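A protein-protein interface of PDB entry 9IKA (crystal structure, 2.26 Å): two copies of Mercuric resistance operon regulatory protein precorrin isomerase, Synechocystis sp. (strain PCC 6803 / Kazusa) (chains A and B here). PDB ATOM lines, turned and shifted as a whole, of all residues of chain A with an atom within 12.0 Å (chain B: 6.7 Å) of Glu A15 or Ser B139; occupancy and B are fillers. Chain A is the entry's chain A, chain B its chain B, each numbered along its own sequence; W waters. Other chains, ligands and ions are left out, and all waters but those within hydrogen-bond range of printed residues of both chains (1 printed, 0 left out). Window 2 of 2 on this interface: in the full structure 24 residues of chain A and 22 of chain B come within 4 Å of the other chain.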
ATOM      1  N   GLN A  14       4.676   1.889 -23.173  1.00  0.00           N
ATOM      2  CA  GLN A  14       5.321   2.007 -24.511  1.00  0.00           C
ATOM      3  C   GLN A  14       6.467   0.998 -24.606  1.00  0.00           C
ATOM      4  O   GLN A  14       7.451   1.096 -23.873  1.00  0.00           O
ATOM      5  CB  GLN A  14       5.827   3.429 -24.760  1.00  0.00           C
ATOM      6  CG  GLN A  14       6.213   3.716 -26.211  1.00  0.00           C
ATOM      7  CD  GLN A  14       5.025   3.882 -27.136  1.00  0.00           C
ATOM      8  OE1 GLN A  14       3.862   3.832 -26.719  1.00  0.00           O
ATOM      9  NE2 GLN A  14       5.305   4.093 -28.414  1.00  0.00           N
ATOM     10  N   GLU A  15       6.315   0.027 -25.514  1.00  0.00           N
ATOM     11  CA  GLU A  15       7.288  -1.033 -25.714  1.00  0.00           C
ATOM     12  C   GLU A  15       7.814  -0.925 -27.144  1.00  0.00           C
ATOM     13  O   GLU A  15       7.675  -1.853 -27.939  1.00  0.00           O
ATOM     14  CB  GLU A  15       6.628  -2.358 -25.321  1.00  0.00           C
ATOM     15  CG  GLU A  15       6.279  -2.410 -23.833  1.00  0.00           C
ATOM     16  CD  GLU A  15       5.399  -3.549 -23.337  1.00  0.00           C
ATOM     17  OE1 GLU A  15       4.835  -4.310 -24.149  1.00  0.00           O
ATOM     18  OE2 GLU A  15       5.285  -3.675 -22.099  1.00  0.00           O
ATOM     19  N   SER A  16       8.399   0.241 -27.445  1.00  0.00           N
ATOM     20  CA  SER A  16       8.984   0.546 -28.743  1.00  0.00           C
ATOM     21  C   SER A  16      10.497   0.677 -28.601  1.00  0.00           C
ATOM     22  O   SER A  16      10.972   1.536 -27.864  1.00  0.00           O
ATOM     23  CB  SER A  16       8.401   1.816 -29.316  1.00  0.00           C
ATOM     24  OG  SER A  16       9.174   2.288 -30.413  1.00  0.00           O
ATOM     25  N   LEU A  17      11.242  -0.161 -29.329  1.00  0.00           N
ATOM     26  CA  LEU A  17      12.689  -0.210 -29.198  1.00  0.00           C
ATOM     27  C   LEU A  17      13.300   1.096 -29.706  1.00  0.00           C
ATOM     28  O   LEU A  17      14.246   1.610 -29.114  1.00  0.00           O
ATOM     29  CB  LEU A  17      13.247  -1.424 -29.941  1.00  0.00           C
ATOM     30  CG  LEU A  17      14.731  -1.727 -29.714  1.00  0.00           C
ATOM     31  CD1 LEU A  17      15.044  -1.923 -28.240  1.00  0.00           C
ATOM     32  CD2 LEU A  17      15.156  -2.945 -30.516  1.00  0.00           C
ATOM     33  N   LYS A  18      12.719   1.637 -30.780  1.00  0.00           N
ATOM     34  CA  LYS A  18      13.185   2.868 -31.401  1.00  0.00           C
ATOM     35  C   LYS A  18      13.192   4.001 -30.371  1.00  0.00           C
ATOM     36  O   LYS A  18      14.145   4.776 -30.302  1.00  0.00           O
ATOM     37  CB  LYS A  18      12.301   3.119 -32.632  1.00  0.00           C
ATOM     38  CG  LYS A  18      12.820   4.086 -33.688  1.00  0.00           C
ATOM     39  CD  LYS A  18      12.318   5.521 -33.561  1.00  0.00           C
ATOM     40  CE  LYS A  18      12.631   6.372 -34.762  1.00  0.00           C
ATOM     41  NZ  LYS A  18      14.069   6.617 -34.915  1.00  0.00           N
ATOM     42  N   HIS A  19      12.147   4.066 -29.537  1.00  0.00           N
ATOM     43  CA  HIS A  19      11.995   5.162 -28.592  1.00  0.00           C
ATOM     44  C   HIS A  19      12.742   4.889 -27.284  1.00  0.00           C
ATOM     45  O   HIS A  19      12.920   5.801 -26.488  1.00  0.00           O
ATOM     46  CB  HIS A  19      10.513   5.498 -28.392  1.00  0.00           C
ATOM     47  CG  HIS A  19       9.822   5.904 -29.658  1.00  0.00           C
ATOM     48  ND1 HIS A  19       9.773   5.101 -30.779  1.00  0.00           N
ATOM     49  CD2 HIS A  19       9.130   7.011 -29.970  1.00  0.00           C
ATOM     50  CE1 HIS A  19       9.087   5.715 -31.733  1.00  0.00           C
ATOM     51  NE2 HIS A  19       8.689   6.879 -31.264  1.00  0.00           N
ATOM     52  N   LEU A  20      13.195   3.648 -27.062  1.00  0.00           N
ATOM     53  CA  LEU A  20      14.028   3.326 -25.909  1.00  0.00           C
ATOM     54  C   LEU A  20      15.490   3.706 -26.164  1.00  0.00           C
ATOM     55  O   LEU A  20      16.167   4.189 -25.261  1.00  0.00           O
ATOM     56  CB  LEU A  20      13.901   1.841 -25.577  1.00  0.00           C
ATOM     57  CG  LEU A  20      14.817   1.325 -24.464  1.00  0.00           C
ATOM     58  CD1 LEU A  20      14.508   2.043 -23.162  1.00  0.00           C
ATOM     59  CD2 LEU A  20      14.700  -0.184 -24.296  1.00  0.00           C
ATOM     60  N   LEU A  21      15.983   3.445 -27.383  1.00  0.00           N
ATOM     61  CA  LEU A  21      17.361   3.746 -27.746  1.00  0.00           C
ATOM     62  C   LEU A  21      17.511   5.222 -28.103  1.00  0.00           C
ATOM     63  O   LEU A  21      16.542   5.891 -28.458  1.00  0.00           O
ATOM     64  CB  LEU A  21      17.777   2.854 -28.913  1.00  0.00           C
ATOM     65  CG  LEU A  21      17.758   1.349 -28.629  1.00  0.00           C
ATOM     66  CD1 LEU A  21      18.124   0.534 -29.859  1.00  0.00           C
ATOM     67  CD2 LEU A  21      18.689   1.034 -27.472  1.00  0.00           C
ATOM     68  N   HIS A  36      20.090  -2.632 -33.309  1.00  0.00           N
ATOM     69  CA  HIS A  36      18.825  -3.033 -32.711  1.00  0.00           C
ATOM     70  C   HIS A  36      18.833  -4.521 -32.364  1.00  0.00           C
ATOM     71  O   HIS A  36      18.396  -4.887 -31.274  1.00  0.00           O
ATOM     72  CB  HIS A  36      17.629  -2.710 -33.619  1.00  0.00           C
ATOM     73  CG  HIS A  36      17.203  -1.278 -33.592  1.00  0.00           C
ATOM     74  ND1 HIS A  36      15.913  -0.887 -33.881  1.00  0.00           N
ATOM     75  CD2 HIS A  36      17.882  -0.154 -33.325  1.00  0.00           C
ATOM     76  CE1 HIS A  36      15.828   0.433 -33.783  1.00  0.00           C
ATOM     77  NE2 HIS A  36      17.011   0.897 -33.450  1.00  0.00           N
ATOM     78  N   VAL A  39      20.987  -5.300 -29.260  1.00  0.00           N
ATOM     79  CA  VAL A  39      20.276  -4.939 -28.043  1.00  0.00           C
ATOM     80  C   VAL A  39      19.220  -5.995 -27.719  1.00  0.00           C
ATOM     81  O   VAL A  39      19.094  -6.381 -26.561  1.00  0.00           O
ATOM     82  CB  VAL A  39      19.661  -3.531 -28.140  1.00  0.00           C
ATOM     83  CG1 VAL A  39      18.594  -3.288 -27.078  1.00  0.00           C
ATOM     84  CG2 VAL A  39      20.738  -2.457 -28.072  1.00  0.00           C
ATOM     85  N   LEU A  40      18.483  -6.465 -28.738  1.00  0.00           N
ATOM     86  CA  LEU A  40      17.445  -7.467 -28.552  1.00  0.00           C
ATOM     87  C   LEU A  40      18.043  -8.783 -28.057  1.00  0.00           C
ATOM     88  O   LEU A  40      17.339  -9.568 -27.436  1.00  0.00           O
ATOM     89  CB  LEU A  40      16.641  -7.715 -29.830  1.00  0.00           C
ATOM     90  CG  LEU A  40      15.607  -6.655 -30.225  1.00  0.00           C
ATOM     91  CD1 LEU A  40      14.875  -7.141 -31.469  1.00  0.00           C
ATOM     92  CD2 LEU A  40      14.610  -6.325 -29.128  1.00  0.00           C
ATOM     93  N   VAL A  45      21.556  -1.701 -23.592  1.00  0.00           N
ATOM     94  CA  VAL A  45      21.341  -0.551 -24.457  1.00  0.00           C
ATOM     95  C   VAL A  45      22.657   0.183 -24.719  1.00  0.00           C
ATOM     96  O   VAL A  45      22.770   0.900 -25.708  1.00  0.00           O
ATOM     97  CB  VAL A  45      20.290   0.409 -23.866  1.00  0.00           C
ATOM     98  CG1 VAL A  45      18.943  -0.278 -23.663  1.00  0.00           C
ATOM     99  CG2 VAL A  45      20.765   1.061 -22.569  1.00  0.00           C
ATOM    100  N   ILE B  98       2.385 -12.954 -29.791  1.00  0.00           N
ATOM    101  CA  ILE B  98       2.336 -11.774 -30.641  1.00  0.00           C
ATOM    102  C   ILE B  98       2.991 -12.117 -31.978  1.00  0.00           C
ATOM    103  O   ILE B  98       4.180 -12.437 -32.018  1.00  0.00           O
ATOM    104  CB  ILE B  98       3.052 -10.591 -29.962  1.00  0.00           C
ATOM    105  CG1 ILE B  98       2.465 -10.287 -28.577  1.00  0.00           C
ATOM    106  CG2 ILE B  98       3.049  -9.351 -30.859  1.00  0.00           C
ATOM    107  CD1 ILE B  98       3.227  -9.230 -27.797  1.00  0.00           C
ATOM    108  N   TRP B 119      -3.132 -10.887 -27.964  1.00  0.00           N
ATOM    109  CA  TRP B 119      -2.221 -11.701 -27.175  1.00  0.00           C
ATOM    110  C   TRP B 119      -2.809 -12.034 -25.803  1.00  0.00           C
ATOM    111  O   TRP B 119      -2.540 -13.105 -25.268  1.00  0.00           O
ATOM    112  CB  TRP B 119      -0.827 -11.061 -27.068  1.00  0.00           C
ATOM    113  CG  TRP B 119      -0.751  -9.728 -26.375  1.00  0.00           C
ATOM    114  CD1 TRP B 119      -0.694  -8.502 -26.969  1.00  0.00           C
ATOM    115  CD2 TRP B 119      -0.674  -9.487 -24.952  1.00  0.00           C
ATOM    116  NE1 TRP B 119      -0.600  -7.515 -26.023  1.00  0.00           N
ATOM    117  CE2 TRP B 119      -0.587  -8.087 -24.777  1.00  0.00           C
ATOM    118  CE3 TRP B 119      -0.684 -10.309 -23.817  1.00  0.00           C
ATOM    119  CZ2 TRP B 119      -0.508  -7.498 -23.515  1.00  0.00           C
ATOM    120  CZ3 TRP B 119      -0.605  -9.725 -22.571  1.00  0.00           C
ATOM    121  CH2 TRP B 119      -0.517  -8.338 -22.423  1.00  0.00           C
ATOM    122  N   LEU B 123      -3.031 -15.685 -24.112  1.00  0.00           N
ATOM    123  CA  LEU B 123      -2.383 -15.905 -22.825  1.00  0.00           C
ATOM    124  C   LEU B 123      -3.346 -16.570 -21.839  1.00  0.00           C
ATOM    125  O   LEU B 123      -2.949 -17.472 -21.103  1.00  0.00           O
ATOM    126  CB  LEU B 123      -1.847 -14.576 -22.293  1.00  0.00           C
ATOM    127  CG  LEU B 123      -1.095 -14.625 -20.958  1.00  0.00           C
ATOM    128  CD1 LEU B 123       0.127 -15.522 -21.002  1.00  0.00           C
ATOM    129  CD2 LEU B 123      -0.696 -13.226 -20.543  1.00  0.00           C
ATOM    130  N   TYR B 136      10.775  -9.947 -24.315  1.00  0.00           N
ATOM    131  CA  TYR B 136      10.609  -8.602 -24.859  1.00  0.00           C
ATOM    132  C   TYR B 136       9.694  -7.737 -23.979  1.00  0.00           C
ATOM    133  O   TYR B 136      10.131  -6.690 -23.508  1.00  0.00           O
ATOM    134  CB  TYR B 136      10.130  -8.658 -26.318  1.00  0.00           C
ATOM    135  CG  TYR B 136      10.083  -7.290 -26.992  1.00  0.00           C
ATOM    136  CD1 TYR B 136      11.238  -6.683 -27.467  1.00  0.00           C
ATOM    137  CD2 TYR B 136       8.887  -6.590 -27.124  1.00  0.00           C
ATOM    138  CE1 TYR B 136      11.207  -5.434 -28.065  1.00  0.00           C
ATOM    139  CE2 TYR B 136       8.841  -5.341 -27.721  1.00  0.00           C
ATOM    140  CZ  TYR B 136      10.004  -4.760 -28.196  1.00  0.00           C
ATOM    141  OH  TYR B 136       9.970  -3.523 -28.782  1.00  0.00           O
ATOM    142  N   ALA B 137       8.439  -8.162 -23.766  1.00  0.00           N
ATOM    143  CA  ALA B 137       7.358  -7.270 -23.347  1.00  0.00           C
ATOM    144  C   ALA B 137       7.024  -7.381 -21.854  1.00  0.00           C
ATOM    145  O   ALA B 137       6.433  -8.370 -21.432  1.00  0.00           O
ATOM    146  CB  ALA B 137       6.129  -7.578 -24.178  1.00  0.00           C
ATOM    147  N   PRO B 138       7.337  -6.364 -21.011  1.00  0.00           N
ATOM    148  CA  PRO B 138       6.884  -6.345 -19.613  1.00  0.00           C
ATOM    149  C   PRO B 138       5.379  -6.520 -19.405  1.00  0.00           C
ATOM    150  O   PRO B 138       4.963  -7.186 -18.458  1.00  0.00           O
ATOM    151  CB  PRO B 138       7.349  -4.971 -19.103  1.00  0.00           C
ATOM    152  CG  PRO B 138       8.526  -4.621 -19.977  1.00  0.00           C
ATOM    153  CD  PRO B 138       8.185  -5.205 -21.339  1.00  0.00           C
ATOM    154  N   SER B 139       4.575  -5.909 -20.288  1.00  0.00           N
ATOM    155  CA  SER B 139       3.122  -5.966 -20.198  1.00  0.00           C
ATOM    156  C   SER B 139       2.615  -7.410 -20.204  1.00  0.00           C
ATOM    157  O   SER B 139       1.630  -7.721 -19.545  1.00  0.00           O
ATOM    158  CB  SER B 139       2.470  -5.160 -21.308  1.00  0.00           C
ATOM    159  OG  SER B 139       2.926  -5.584 -22.588  1.00  0.00           O
ATOM    160  N   VAL B 140       3.278  -8.285 -20.961  1.00  0.00           N
ATOM    161  CA  VAL B 140       2.900  -9.689 -21.037  1.00  0.00           C
ATOM    162  C   VAL B 140       3.202 -10.379 -19.708  1.00  0.00           C
ATOM    163  O   VAL B 140       2.444 -11.243 -19.272  1.00  0.00           O
ATOM    164  CB  VAL B 140       3.626 -10.401 -22.197  1.00  0.00           C
ATOM    165  CG1 VAL B 140       3.348 -11.902 -22.205  1.00  0.00           C
ATOM    166  CG2 VAL B 140       3.268  -9.782 -23.542  1.00  0.00           C
ATOM    167  N   LEU B 141       4.324  -9.999 -19.086  1.00  0.00           N
ATOM    168  CA  LEU B 141       4.739 -10.564 -17.811  1.00  0.00           C
ATOM    169  C   LEU B 141       3.801 -10.105 -16.690  1.00  0.00           C
ATOM    170  O   LEU B 141       3.453 -10.905 -15.818  1.00  0.00           O
ATOM    171  CB  LEU B 141       6.196 -10.183 -17.535  1.00  0.00           C
ATOM    172  CG  LEU B 141       6.789 -10.703 -16.222  1.00  0.00           C
ATOM    173  CD1 LEU B 141       6.694 -12.223 -16.135  1.00  0.00           C
ATOM    174  CD2 LEU B 141       8.229 -10.226 -16.067  1.00  0.00           C
ATOM    175  N   LEU B 142       3.412  -8.820 -16.716  1.00  0.00           N
ATOM    176  CA  LEU B 142       2.479  -8.260 -15.746  1.00  0.00           C
ATOM    177  C   LEU B 142       1.145  -9.000 -15.810  1.00  0.00           C
ATOM    178  O   LEU B 142       0.633  -9.428 -14.781  1.00  0.00           O
ATOM    179  CB  LEU B 142       2.270  -6.759 -15.956  1.00  0.00           C
ATOM    180  CG  LEU B 142       3.316  -5.839 -15.319  1.00  0.00           C
ATOM    181  CD1 LEU B 142       3.341  -4.468 -15.988  1.00  0.00           C
ATOM    182  CD2 LEU B 142       3.065  -5.692 -13.825  1.00  0.00           C
ATOM    183  N   THR B 143       0.576  -9.135 -17.016  1.00  0.00           N
ATOM    184  CA  THR B 143      -0.700  -9.816 -17.175  1.00  0.00           C
ATOM    185  C   THR B 143      -0.566 -11.271 -16.716  1.00  0.00           C
ATOM    186  O   THR B 143      -1.440 -11.786 -16.028  1.00  0.00           O
ATOM    187  CB  THR B 143      -1.198  -9.702 -18.616  1.00  0.00           C
ATOM    188  OG1 THR B 143      -1.365  -8.315 -18.881  1.00  0.00           O
ATOM    189  CG2 THR B 143      -2.553 -10.354 -18.823  1.00  0.00           C
ATOM    190  N   ALA B 144       0.537 -11.929 -17.076  1.00  0.00           N
ATOM    191  CA  ALA B 144       0.742 -13.317 -16.689  1.00  0.00           C
ATOM    192  C   ALA B 144       0.732 -13.457 -15.167  1.00  0.00           C
ATOM    193  O   ALA B 144       0.088 -14.361 -14.647  1.00  0.00           O
ATOM    194  CB  ALA B 144       2.022 -13.850 -17.294  1.00  0.00           C
ATOM    195  N   PRO B 162      12.222  -9.704 -19.854  1.00  0.00           N
ATOM    196  CA  PRO B 162      11.920  -8.633 -20.807  1.00  0.00           C
ATOM    197  C   PRO B 162      13.039  -7.602 -20.943  1.00  0.00           C
ATOM    198  O   PRO B 162      13.899  -7.471 -20.069  1.00  0.00           O
ATOM    199  CB  PRO B 162      10.641  -8.015 -20.239  1.00  0.00           C
ATOM    200  CG  PRO B 162      10.762  -8.253 -18.752  1.00  0.00           C
ATOM    201  CD  PRO B 162      11.377  -9.639 -18.651  1.00  0.00           C
ATOM    202  N   PHE B 165      12.325  -1.740 -20.794  1.00  0.00           N
ATOM    203  CA  PHE B 165      11.365  -0.654 -20.899  1.00  0.00           C
ATOM    204  C   PHE B 165      10.961  -0.187 -19.496  1.00  0.00           C
ATOM    205  O   PHE B 165      11.309  -0.813 -18.496  1.00  0.00           O
ATOM    206  CB  PHE B 165      10.174  -1.133 -21.730  1.00  0.00           C
ATOM    207  CG  PHE B 165      10.507  -1.543 -23.157  1.00  0.00           C
ATOM    208  CD1 PHE B 165      10.732  -0.582 -24.139  1.00  0.00           C
ATOM    209  CD2 PHE B 165      10.536  -2.885 -23.528  1.00  0.00           C
ATOM    210  CE1 PHE B 165      11.013  -0.960 -25.444  1.00  0.00           C
ATOM    211  CE2 PHE B 165      10.804  -3.256 -24.836  1.00  0.00           C
ATOM    212  CZ  PHE B 165      11.054  -2.293 -25.788  1.00  0.00           C
ATOM    213  N   HIS B 167       8.369  -0.197 -17.605  1.00  0.00           N
ATOM    214  CA  HIS B 167       7.576  -1.026 -16.704  1.00  0.00           C
ATOM    215  C   HIS B 167       8.261  -2.356 -16.363  1.00  0.00           C
ATOM    216  O   HIS B 167       7.680  -3.173 -15.654  1.00  0.00           O
ATOM    217  CB  HIS B 167       6.175  -1.252 -17.288  1.00  0.00           C
ATOM    218  CG  HIS B 167       5.280  -0.061 -17.194  1.00  0.00           C
ATOM    219  ND1 HIS B 167       3.908  -0.167 -17.097  1.00  0.00           N
ATOM    220  CD2 HIS B 167       5.551   1.255 -17.157  1.00  0.00           C
ATOM    221  CE1 HIS B 167       3.377   1.046 -17.014  1.00  0.00           C
ATOM    222  NE2 HIS B 167       4.357   1.927 -17.047  1.00  0.00           N
ATOM    223  N   ALA B 171       7.489  -5.349 -13.317  1.00  0.00           N
ATOM    224  CA  ALA B 171       6.991  -6.630 -13.789  1.00  0.00           C
ATOM    225  C   ALA B 171       7.802  -7.770 -13.179  1.00  0.00           C
ATOM    226  O   ALA B 171       7.243  -8.784 -12.778  1.00  0.00           O
ATOM    227  CB  ALA B 171       7.038  -6.679 -15.301  1.00  0.00           C
HETATM  228  O   HOH W   1       6.866  -1.131 -20.378  1.00  0.00           O
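The side-chain hydroxyl of Tyr B136 sits at hydrogen-bond distance from the backbone carbonyl oxygen of Glu A15, 3.0 Å away. The side-chain carboxylate (OE1) of Glu A15 sits at hydrogen-bond distance from the side-chain hydroxyl (OG) of Ser B139, 2.8 Å away.
A ring nitrogen (ND1) of His A19 is in hydrogen-bond range of the side-chain hydroxyl of Ser A16, at 2.9 Å. The side-chain hydroxyl (OG1) of Thr B143 lies within hydrogen-bond range of the backbone carbonyl oxygen (O) of Ser B139 (3.1 Å).
Among the printed residues, merely in contact across the chains: Gln A14 with Phe B165 (3.7 Å), Glu A15 with Ala B137 (3.5 Å), Glu A15 with Pro B138 (3.4 Å), Glu A15 with Phe B165 (3.6 Å), Ser A16 with Phe B165 (3.5 Å), Leu A17 with Tyr B136 (3.6 Å), Leu A17 with Phe B165 (3.97 Å), Leu A20 with Phe B165 (3.9 Å) and Leu A40 with Tyr B136 (3.7 Å).
Of chain A, only Glu A15 comes within 4 Å of Ser B139. Ala B137 touches just one residue of chain A: Glu A15. Val B140 touches none of the printed residues of chain A. No residue of chain A comes within 4 Å of Leu B141. Leu B142 touches none of the printed residues of chain A. Of chain A, only Gln A14, Glu A15, Ser A16, Leu A17 and Leu A20 come within 4 Å of Phe B165. Of the printed residues of chain B, Leu A40 touches Tyr B136 (3.7 Å). Of the printed residues of chain B, Leu A17 touches Tyr B136 (3.6 Å) and Phe B165 (3.97 Å). Of the printed residues of chain B, Ser A16 touches Phe B165 (3.5 Å). Printed residues of chain B within 4 Å of Gln A14: Phe B165. Ala B171 touches none of the printed residues of chain A. His A36 touches none of the printed residues of chain B. The nearest residue of chain A that does not touch Ser B139 is Gln A14 (7.6 Å). The nearest printed residue of chain A that does not touch Tyr B136 is Ser A16 (4.2 Å).
Of the 16 printed residues of chain B, 5 touch a printed residue of chain A. Printed residues of chain B that touch a printed residue of chain A: Tyr B136, Ala B137, Pro B138, Ser B139 and Phe B165. Among the printed residues, no Asp or Glu carboxylate lies within 4 Å of a Lys or Arg side-chain nitrogen of the other chain.
No position is printed for both chains. Of the 11 pairs that touch across the chains among the printed residues, none has its exchanged pair printed and touching as well.
Water W1 lies within hydrogen-bond range of the backbone NH (N) of His B167 (3.3 Å) and the side-chain carboxylate (OE2) of Glu A15 (3.5 Å).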
